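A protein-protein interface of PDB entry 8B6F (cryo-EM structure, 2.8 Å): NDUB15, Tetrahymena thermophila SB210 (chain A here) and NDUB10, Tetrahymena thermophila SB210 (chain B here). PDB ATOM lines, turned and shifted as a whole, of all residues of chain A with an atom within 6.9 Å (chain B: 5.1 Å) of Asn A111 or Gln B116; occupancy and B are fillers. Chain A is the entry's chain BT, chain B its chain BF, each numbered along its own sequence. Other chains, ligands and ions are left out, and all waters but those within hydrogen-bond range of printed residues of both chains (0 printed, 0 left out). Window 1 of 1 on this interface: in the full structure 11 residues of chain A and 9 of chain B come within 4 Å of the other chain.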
ATOM      1  N   GLY A 103      34.201 -15.939  19.391  1.00  0.00           N
ATOM      2  CA  GLY A 103      34.737 -17.279  19.285  1.00  0.00           C
ATOM      3  C   GLY A 103      33.899 -18.300  20.030  1.00  0.00           C
ATOM      4  O   GLY A 103      32.766 -18.046  20.442  1.00  0.00           O
ATOM      5  N   THR A 104      34.483 -19.484  20.200  1.00  0.00           N
ATOM      6  CA  THR A 104      33.777 -20.569  20.865  1.00  0.00           C
ATOM      7  C   THR A 104      33.412 -20.172  22.291  1.00  0.00           C
ATOM      8  O   THR A 104      34.242 -19.642  23.034  1.00  0.00           O
ATOM      9  CB  THR A 104      34.633 -21.836  20.866  1.00  0.00           C
ATOM     10  OG1 THR A 104      34.980 -22.182  19.518  1.00  0.00           O
ATOM     11  CG2 THR A 104      33.880 -23.001  21.492  1.00  0.00           C
ATOM     12  N   SER A 105      32.168 -20.439  22.667  1.00  0.00           N
ATOM     13  CA  SER A 105      31.647 -20.156  23.992  1.00  0.00           C
ATOM     14  C   SER A 105      31.284 -21.463  24.683  1.00  0.00           C
ATOM     15  O   SER A 105      31.047 -22.486  24.038  1.00  0.00           O
ATOM     16  CB  SER A 105      30.416 -19.246  23.918  1.00  0.00           C
ATOM     17  OG  SER A 105      29.945 -18.918  25.213  1.00  0.00           O
ATOM     18  N   PHE A 108      26.264 -25.898  25.116  1.00  0.00           N
ATOM     19  CA  PHE A 108      25.945 -27.166  24.458  1.00  0.00           C
ATOM     20  C   PHE A 108      25.387 -26.851  23.076  1.00  0.00           C
ATOM     21  O   PHE A 108      24.179 -26.717  22.885  1.00  0.00           O
ATOM     22  CB  PHE A 108      24.957 -27.979  25.286  1.00  0.00           C
ATOM     23  CG  PHE A 108      25.477 -28.369  26.637  1.00  0.00           C
ATOM     24  CD1 PHE A 108      25.321 -27.527  27.725  1.00  0.00           C
ATOM     25  CD2 PHE A 108      26.121 -29.581  26.822  1.00  0.00           C
ATOM     26  CE1 PHE A 108      25.800 -27.883  28.969  1.00  0.00           C
ATOM     27  CE2 PHE A 108      26.602 -29.945  28.064  1.00  0.00           C
ATOM     28  CZ  PHE A 108      26.441 -29.095  29.139  1.00  0.00           C
ATOM     29  N   TYR A 109      26.282 -26.728  22.101  1.00  0.00           N
ATOM     30  CA  TYR A 109      25.860 -26.424  20.742  1.00  0.00           C
ATOM     31  C   TYR A 109      24.985 -27.541  20.192  1.00  0.00           C
ATOM     32  O   TYR A 109      25.179 -28.721  20.496  1.00  0.00           O
ATOM     33  CB  TYR A 109      27.071 -26.219  19.839  1.00  0.00           C
ATOM     34  CG  TYR A 109      27.853 -24.985  20.188  1.00  0.00           C
ATOM     35  CD1 TYR A 109      27.404 -23.727  19.814  1.00  0.00           C
ATOM     36  CD2 TYR A 109      29.040 -25.077  20.895  1.00  0.00           C
ATOM     37  CE1 TYR A 109      28.113 -22.599  20.133  1.00  0.00           C
ATOM     38  CE2 TYR A 109      29.754 -23.958  21.216  1.00  0.00           C
ATOM     39  CZ  TYR A 109      29.288 -22.724  20.832  1.00  0.00           C
ATOM     40  OH  TYR A 109      30.022 -21.628  21.169  1.00  0.00           O
ATOM     41  N   HIS A 110      24.008 -27.156  19.378  1.00  0.00           N
ATOM     42  CA  HIS A 110      22.990 -28.069  18.875  1.00  0.00           C
ATOM     43  C   HIS A 110      22.859 -27.933  17.364  1.00  0.00           C
ATOM     44  O   HIS A 110      21.763 -27.801  16.817  1.00  0.00           O
ATOM     45  CB  HIS A 110      21.659 -27.809  19.570  1.00  0.00           C
ATOM     46  CG  HIS A 110      20.711 -28.964  19.501  1.00  0.00           C
ATOM     47  ND1 HIS A 110      19.790 -29.112  18.486  1.00  0.00           N
ATOM     48  CD2 HIS A 110      20.546 -30.031  20.317  1.00  0.00           C
ATOM     49  CE1 HIS A 110      19.096 -30.217  18.682  1.00  0.00           C
ATOM     50  NE2 HIS A 110      19.534 -30.795  19.785  1.00  0.00           N
ATOM     51  N   ASN A 111      23.996 -27.955  16.664  1.00  0.00           N
ATOM     52  CA  ASN A 111      23.964 -27.841  15.209  1.00  0.00           C
ATOM     53  C   ASN A 111      23.182 -28.989  14.591  1.00  0.00           C
ATOM     54  O   ASN A 111      22.368 -28.784  13.684  1.00  0.00           O
ATOM     55  CB  ASN A 111      25.383 -27.813  14.640  1.00  0.00           C
ATOM     56  CG  ASN A 111      26.343 -27.027  15.503  1.00  0.00           C
ATOM     57  OD1 ASN A 111      26.109 -25.860  15.814  1.00  0.00           O
ATOM     58  ND2 ASN A 111      27.428 -27.672  15.907  1.00  0.00           N
ATOM     59  N   ASN A 112      23.427 -30.208  15.061  1.00  0.00           N
ATOM     60  CA  ASN A 112      22.690 -31.370  14.590  1.00  0.00           C
ATOM     61  C   ASN A 112      21.360 -31.466  15.321  1.00  0.00           C
ATOM     62  O   ASN A 112      21.313 -31.411  16.553  1.00  0.00           O
ATOM     63  CB  ASN A 112      23.505 -32.641  14.815  1.00  0.00           C
ATOM     64  CG  ASN A 112      24.959 -32.481  14.428  1.00  0.00           C
ATOM     65  OD1 ASN A 112      25.434 -31.369  14.205  1.00  0.00           O
ATOM     66  ND2 ASN A 112      25.678 -33.594  14.351  1.00  0.00           N
ATOM     67  N   ALA A 113      20.276 -31.616  14.562  1.00  0.00           N
ATOM     68  CA  ALA A 113      18.934 -31.692  15.136  1.00  0.00           C
ATOM     69  C   ALA A 113      18.714 -33.087  15.724  1.00  0.00           C
ATOM     70  O   ALA A 113      17.825 -33.838  15.325  1.00  0.00           O
ATOM     71  CB  ALA A 113      17.887 -31.355  14.086  1.00  0.00           C
ATOM     72  N   GLY A 114      19.552 -33.423  16.702  1.00  0.00           N
ATOM     73  CA  GLY A 114      19.487 -34.723  17.328  1.00  0.00           C
ATOM     74  C   GLY A 114      20.063 -35.837  16.487  1.00  0.00           C
ATOM     75  O   GLY A 114      19.912 -37.009  16.847  1.00  0.00           O
ATOM     76  N   PHE A 115      20.721 -35.506  15.379  1.00  0.00           N
ATOM     77  CA  PHE A 115      21.307 -36.498  14.485  1.00  0.00           C
ATOM     78  C   PHE A 115      22.681 -36.885  15.014  1.00  0.00           C
ATOM     79  O   PHE A 115      23.613 -36.075  14.999  1.00  0.00           O
ATOM     80  CB  PHE A 115      21.404 -35.944  13.066  1.00  0.00           C
ATOM     81  CG  PHE A 115      20.075 -35.716  12.407  1.00  0.00           C
ATOM     82  CD1 PHE A 115      19.102 -36.700  12.417  1.00  0.00           C
ATOM     83  CD2 PHE A 115      19.798 -34.515  11.778  1.00  0.00           C
ATOM     84  CE1 PHE A 115      17.880 -36.493  11.812  1.00  0.00           C
ATOM     85  CE2 PHE A 115      18.578 -34.301  11.172  1.00  0.00           C
ATOM     86  CZ  PHE A 115      17.618 -35.291  11.187  1.00  0.00           C
ATOM     87  N   TYR B  44      19.322 -24.272  12.826  1.00  0.00           N
ATOM     88  CA  TYR B  44      19.601 -23.166  11.914  1.00  0.00           C
ATOM     89  C   TYR B  44      18.422 -22.888  10.993  1.00  0.00           C
ATOM     90  O   TYR B  44      18.052 -21.728  10.783  1.00  0.00           O
ATOM     91  CB  TYR B  44      20.851 -23.475  11.089  1.00  0.00           C
ATOM     92  CG  TYR B  44      22.154 -23.369  11.848  1.00  0.00           C
ATOM     93  CD1 TYR B  44      22.415 -22.287  12.679  1.00  0.00           C
ATOM     94  CD2 TYR B  44      23.126 -24.352  11.728  1.00  0.00           C
ATOM     95  CE1 TYR B  44      23.609 -22.187  13.369  1.00  0.00           C
ATOM     96  CE2 TYR B  44      24.321 -24.262  12.413  1.00  0.00           C
ATOM     97  CZ  TYR B  44      24.556 -23.177  13.232  1.00  0.00           C
ATOM     98  OH  TYR B  44      25.746 -23.088  13.914  1.00  0.00           O
ATOM     99  N   TYR B  53      16.630 -30.886   6.495  1.00  0.00           N
ATOM    100  CA  TYR B  53      17.604 -30.379   7.452  1.00  0.00           C
ATOM    101  C   TYR B  53      18.747 -31.357   7.675  1.00  0.00           C
ATOM    102  O   TYR B  53      19.865 -30.933   7.985  1.00  0.00           O
ATOM    103  CB  TYR B  53      16.945 -30.051   8.789  1.00  0.00           C
ATOM    104  CG  TYR B  53      17.931 -29.434   9.748  1.00  0.00           C
ATOM    105  CD1 TYR B  53      18.214 -28.076   9.703  1.00  0.00           C
ATOM    106  CD2 TYR B  53      18.615 -30.216  10.668  1.00  0.00           C
ATOM    107  CE1 TYR B  53      19.132 -27.511  10.563  1.00  0.00           C
ATOM    108  CE2 TYR B  53      19.533 -29.660  11.531  1.00  0.00           C
ATOM    109  CZ  TYR B  53      19.788 -28.308  11.474  1.00  0.00           C
ATOM    110  OH  TYR B  53      20.702 -27.752  12.333  1.00  0.00           O
ATOM    111  N   LYS B  57      22.442 -30.168   7.259  1.00  0.00           N
ATOM    112  CA  LYS B  57      23.500 -30.419   8.230  1.00  0.00           C
ATOM    113  C   LYS B  57      24.710 -31.067   7.572  1.00  0.00           C
ATOM    114  O   LYS B  57      25.851 -30.677   7.835  1.00  0.00           O
ATOM    115  CB  LYS B  57      22.959 -31.304   9.353  1.00  0.00           C
ATOM    116  CG  LYS B  57      24.001 -31.771  10.359  1.00  0.00           C
ATOM    117  CD  LYS B  57      23.453 -32.877  11.247  1.00  0.00           C
ATOM    118  CE  LYS B  57      23.322 -34.201  10.506  1.00  0.00           C
ATOM    119  NZ  LYS B  57      24.632 -34.712  10.019  1.00  0.00           N
ATOM    120  N   ARG B 111      37.291 -22.837  10.304  1.00  0.00           N
ATOM    121  CA  ARG B 111      37.459 -23.444  11.623  1.00  0.00           C
ATOM    122  C   ARG B 111      38.558 -24.491  11.513  1.00  0.00           C
ATOM    123  O   ARG B 111      38.310 -25.654  11.194  1.00  0.00           O
ATOM    124  CB  ARG B 111      36.146 -24.042  12.104  1.00  0.00           C
ATOM    125  CG  ARG B 111      36.223 -24.795  13.425  1.00  0.00           C
ATOM    126  CD  ARG B 111      35.248 -25.959  13.441  1.00  0.00           C
ATOM    127  NE  ARG B 111      35.588 -26.960  12.438  1.00  0.00           N
ATOM    128  CZ  ARG B 111      34.786 -27.943  12.054  1.00  0.00           C
ATOM    129  NH1 ARG B 111      33.574 -28.085  12.561  1.00  0.00           N
ATOM    130  NH2 ARG B 111      35.213 -28.807  11.138  1.00  0.00           N
ATOM    131  N   HIS B 114      39.244 -25.503  16.029  1.00  0.00           N
ATOM    132  CA  HIS B 114      38.338 -25.128  17.100  1.00  0.00           C
ATOM    133  C   HIS B 114      37.201 -26.137  17.203  1.00  0.00           C
ATOM    134  O   HIS B 114      36.785 -26.741  16.213  1.00  0.00           O
ATOM    135  CB  HIS B 114      37.781 -23.728  16.857  1.00  0.00           C
ATOM    136  CG  HIS B 114      38.833 -22.711  16.546  1.00  0.00           C
ATOM    137  ND1 HIS B 114      40.166 -22.905  16.839  1.00  0.00           N
ATOM    138  CD2 HIS B 114      38.752 -21.496  15.956  1.00  0.00           C
ATOM    139  CE1 HIS B 114      40.859 -21.853  16.447  1.00  0.00           C
ATOM    140  NE2 HIS B 114      40.026 -20.982  15.909  1.00  0.00           N
ATOM    141  N   PHE B 115      36.702 -26.320  18.426  1.00  0.00           N
ATOM    142  CA  PHE B 115      35.622 -27.274  18.640  1.00  0.00           C
ATOM    143  C   PHE B 115      34.400 -26.917  17.806  1.00  0.00           C
ATOM    144  O   PHE B 115      33.776 -27.795  17.198  1.00  0.00           O
ATOM    145  CB  PHE B 115      35.251 -27.326  20.124  1.00  0.00           C
ATOM    146  CG  PHE B 115      36.215 -28.109  20.978  1.00  0.00           C
ATOM    147  CD1 PHE B 115      36.844 -29.246  20.495  1.00  0.00           C
ATOM    148  CD2 PHE B 115      36.470 -27.714  22.279  1.00  0.00           C
ATOM    149  CE1 PHE B 115      37.717 -29.963  21.289  1.00  0.00           C
ATOM    150  CE2 PHE B 115      37.340 -28.426  23.078  1.00  0.00           C
ATOM    151  CZ  PHE B 115      37.965 -29.554  22.584  1.00  0.00           C
ATOM    152  N   GLN B 116      34.041 -25.637  17.762  1.00  0.00           N
ATOM    153  CA  GLN B 116      32.847 -25.183  17.069  1.00  0.00           C
ATOM    154  C   GLN B 116      33.164 -23.951  16.240  1.00  0.00           C
ATOM    155  O   GLN B 116      33.858 -23.041  16.702  1.00  0.00           O
ATOM    156  CB  GLN B 116      31.724 -24.857  18.061  1.00  0.00           C
ATOM    157  CG  GLN B 116      30.420 -24.420  17.412  1.00  0.00           C
ATOM    158  CD  GLN B 116      29.696 -25.563  16.736  1.00  0.00           C
ATOM    159  OE1 GLN B 116      28.744 -26.115  17.283  1.00  0.00           O
ATOM    160  NE2 GLN B 116      30.137 -25.921  15.536  1.00  0.00           N
ATOM    161  N   ALA B 117      32.653 -23.930  15.013  1.00  0.00           N
ATOM    162  CA  ALA B 117      32.669 -22.736  14.177  1.00  0.00           C
ATOM    163  C   ALA B 117      31.420 -21.928  14.501  1.00  0.00           C
ATOM    164  O   ALA B 117      30.311 -22.309  14.115  1.00  0.00           O
ATOM    165  CB  ALA B 117      32.708 -23.111  12.698  1.00  0.00           C
ATOM    166  N   VAL B 118      31.597 -20.810  15.200  1.00  0.00           N
ATOM    167  CA  VAL B 118      30.462 -20.018  15.657  1.00  0.00           C
ATOM    168  C   VAL B 118      29.868 -19.288  14.463  1.00  0.00           C
ATOM    169  O   VAL B 118      30.373 -18.243  14.041  1.00  0.00           O
ATOM    170  CB  VAL B 118      30.877 -19.037  16.767  1.00  0.00           C
ATOM    171  CG1 VAL B 118      29.715 -18.131  17.152  1.00  0.00           C
ATOM    172  CG2 VAL B 118      31.378 -19.802  17.978  1.00  0.00           C
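The backbone carbonyl oxygen of Gln B116 is in hydrogen-bond range of the side-chain hydroxyl of Thr A104. The side-chain hydroxyl (OH) of Tyr B44 lies within hydrogen-bond range of the side-chain amide oxygen (OD1) of Asn A111 (3.4 Å). OE1 of Gln B116 is in hydrogen-bond range of ND2 of Asn A111. The backbone carbonyl oxygen (O) of Asn A111 sits close to the side-chain hydroxyl (OH) of Tyr B53 (2.4 Å).
The backbone carbonyl oxygen (O) of Phe A115 is in hydrogen-bond range of the side-chain amide nitrogen (ND2) of Asn A112 (3.3 Å). N of Ser A105 sits at hydrogen-bond distance from OH of Tyr A109, at 2.9 Å. A ring nitrogen (ND1) of His A110 sits close to the backbone carbonyl oxygen (O) of Asn A112, at 3.4 Å.
Phe A108 touches none of the printed residues of chain B. Of chain B, only Tyr B44 (3.4 Å), Tyr B53 (2.4 Å) and Gln B116 (2.5 Å) come within 4 Å of Asn A111. Of the printed residues of chain A, Tyr B53 touches Asn A111 (2.4 Å) and Ala A113 (3.5 Å). Printed residues of chain A within 4 Å of Lys B57: Asn A112 and Phe A115. Arg B111 touches none of the printed residues of chain A. Gln B116 touches just these residues of chain A: Thr A104, Tyr A109 and Asn A111. Of the printed residues of chain A, Val B118 touches Gly A103, Thr A104 and Tyr A109. The nearest residue of chain B that does not touch Asn A111 is Lys B57 (4.8 Å). The nearest residue of chain A that does not touch Gln B116 is His A110 (5.3 Å).
Among the printed residues, pairs that only touch across the chains: Tyr A109 with Gln B116 (3.1 Å), Gly A103 with Val B118 (3.3 Å), Ala A113 with Tyr B53 (3.5 Å), Asn A112 with Lys B57 (3.5 Å), Phe A115 with Lys B57 (3.6 Å), Thr A104 with Val B118 (3.8 Å) and Tyr A109 with Val B118 (3.9 Å).
Printed residues of chain A that touch a printed residue of chain B: Gly A103, Thr A104, Tyr A109, Asn A111, Asn A112, Ala A113 and Phe A115. Of the 9 printed residues of chain B, 5 touch a printed residue of chain A. Among the printed residues, 11 pairs touch across the chains. Among the printed residues, no Asp or Glu carboxylate lies within 4 Å of a Lys or Arg side-chain nitrogen of the other chain.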
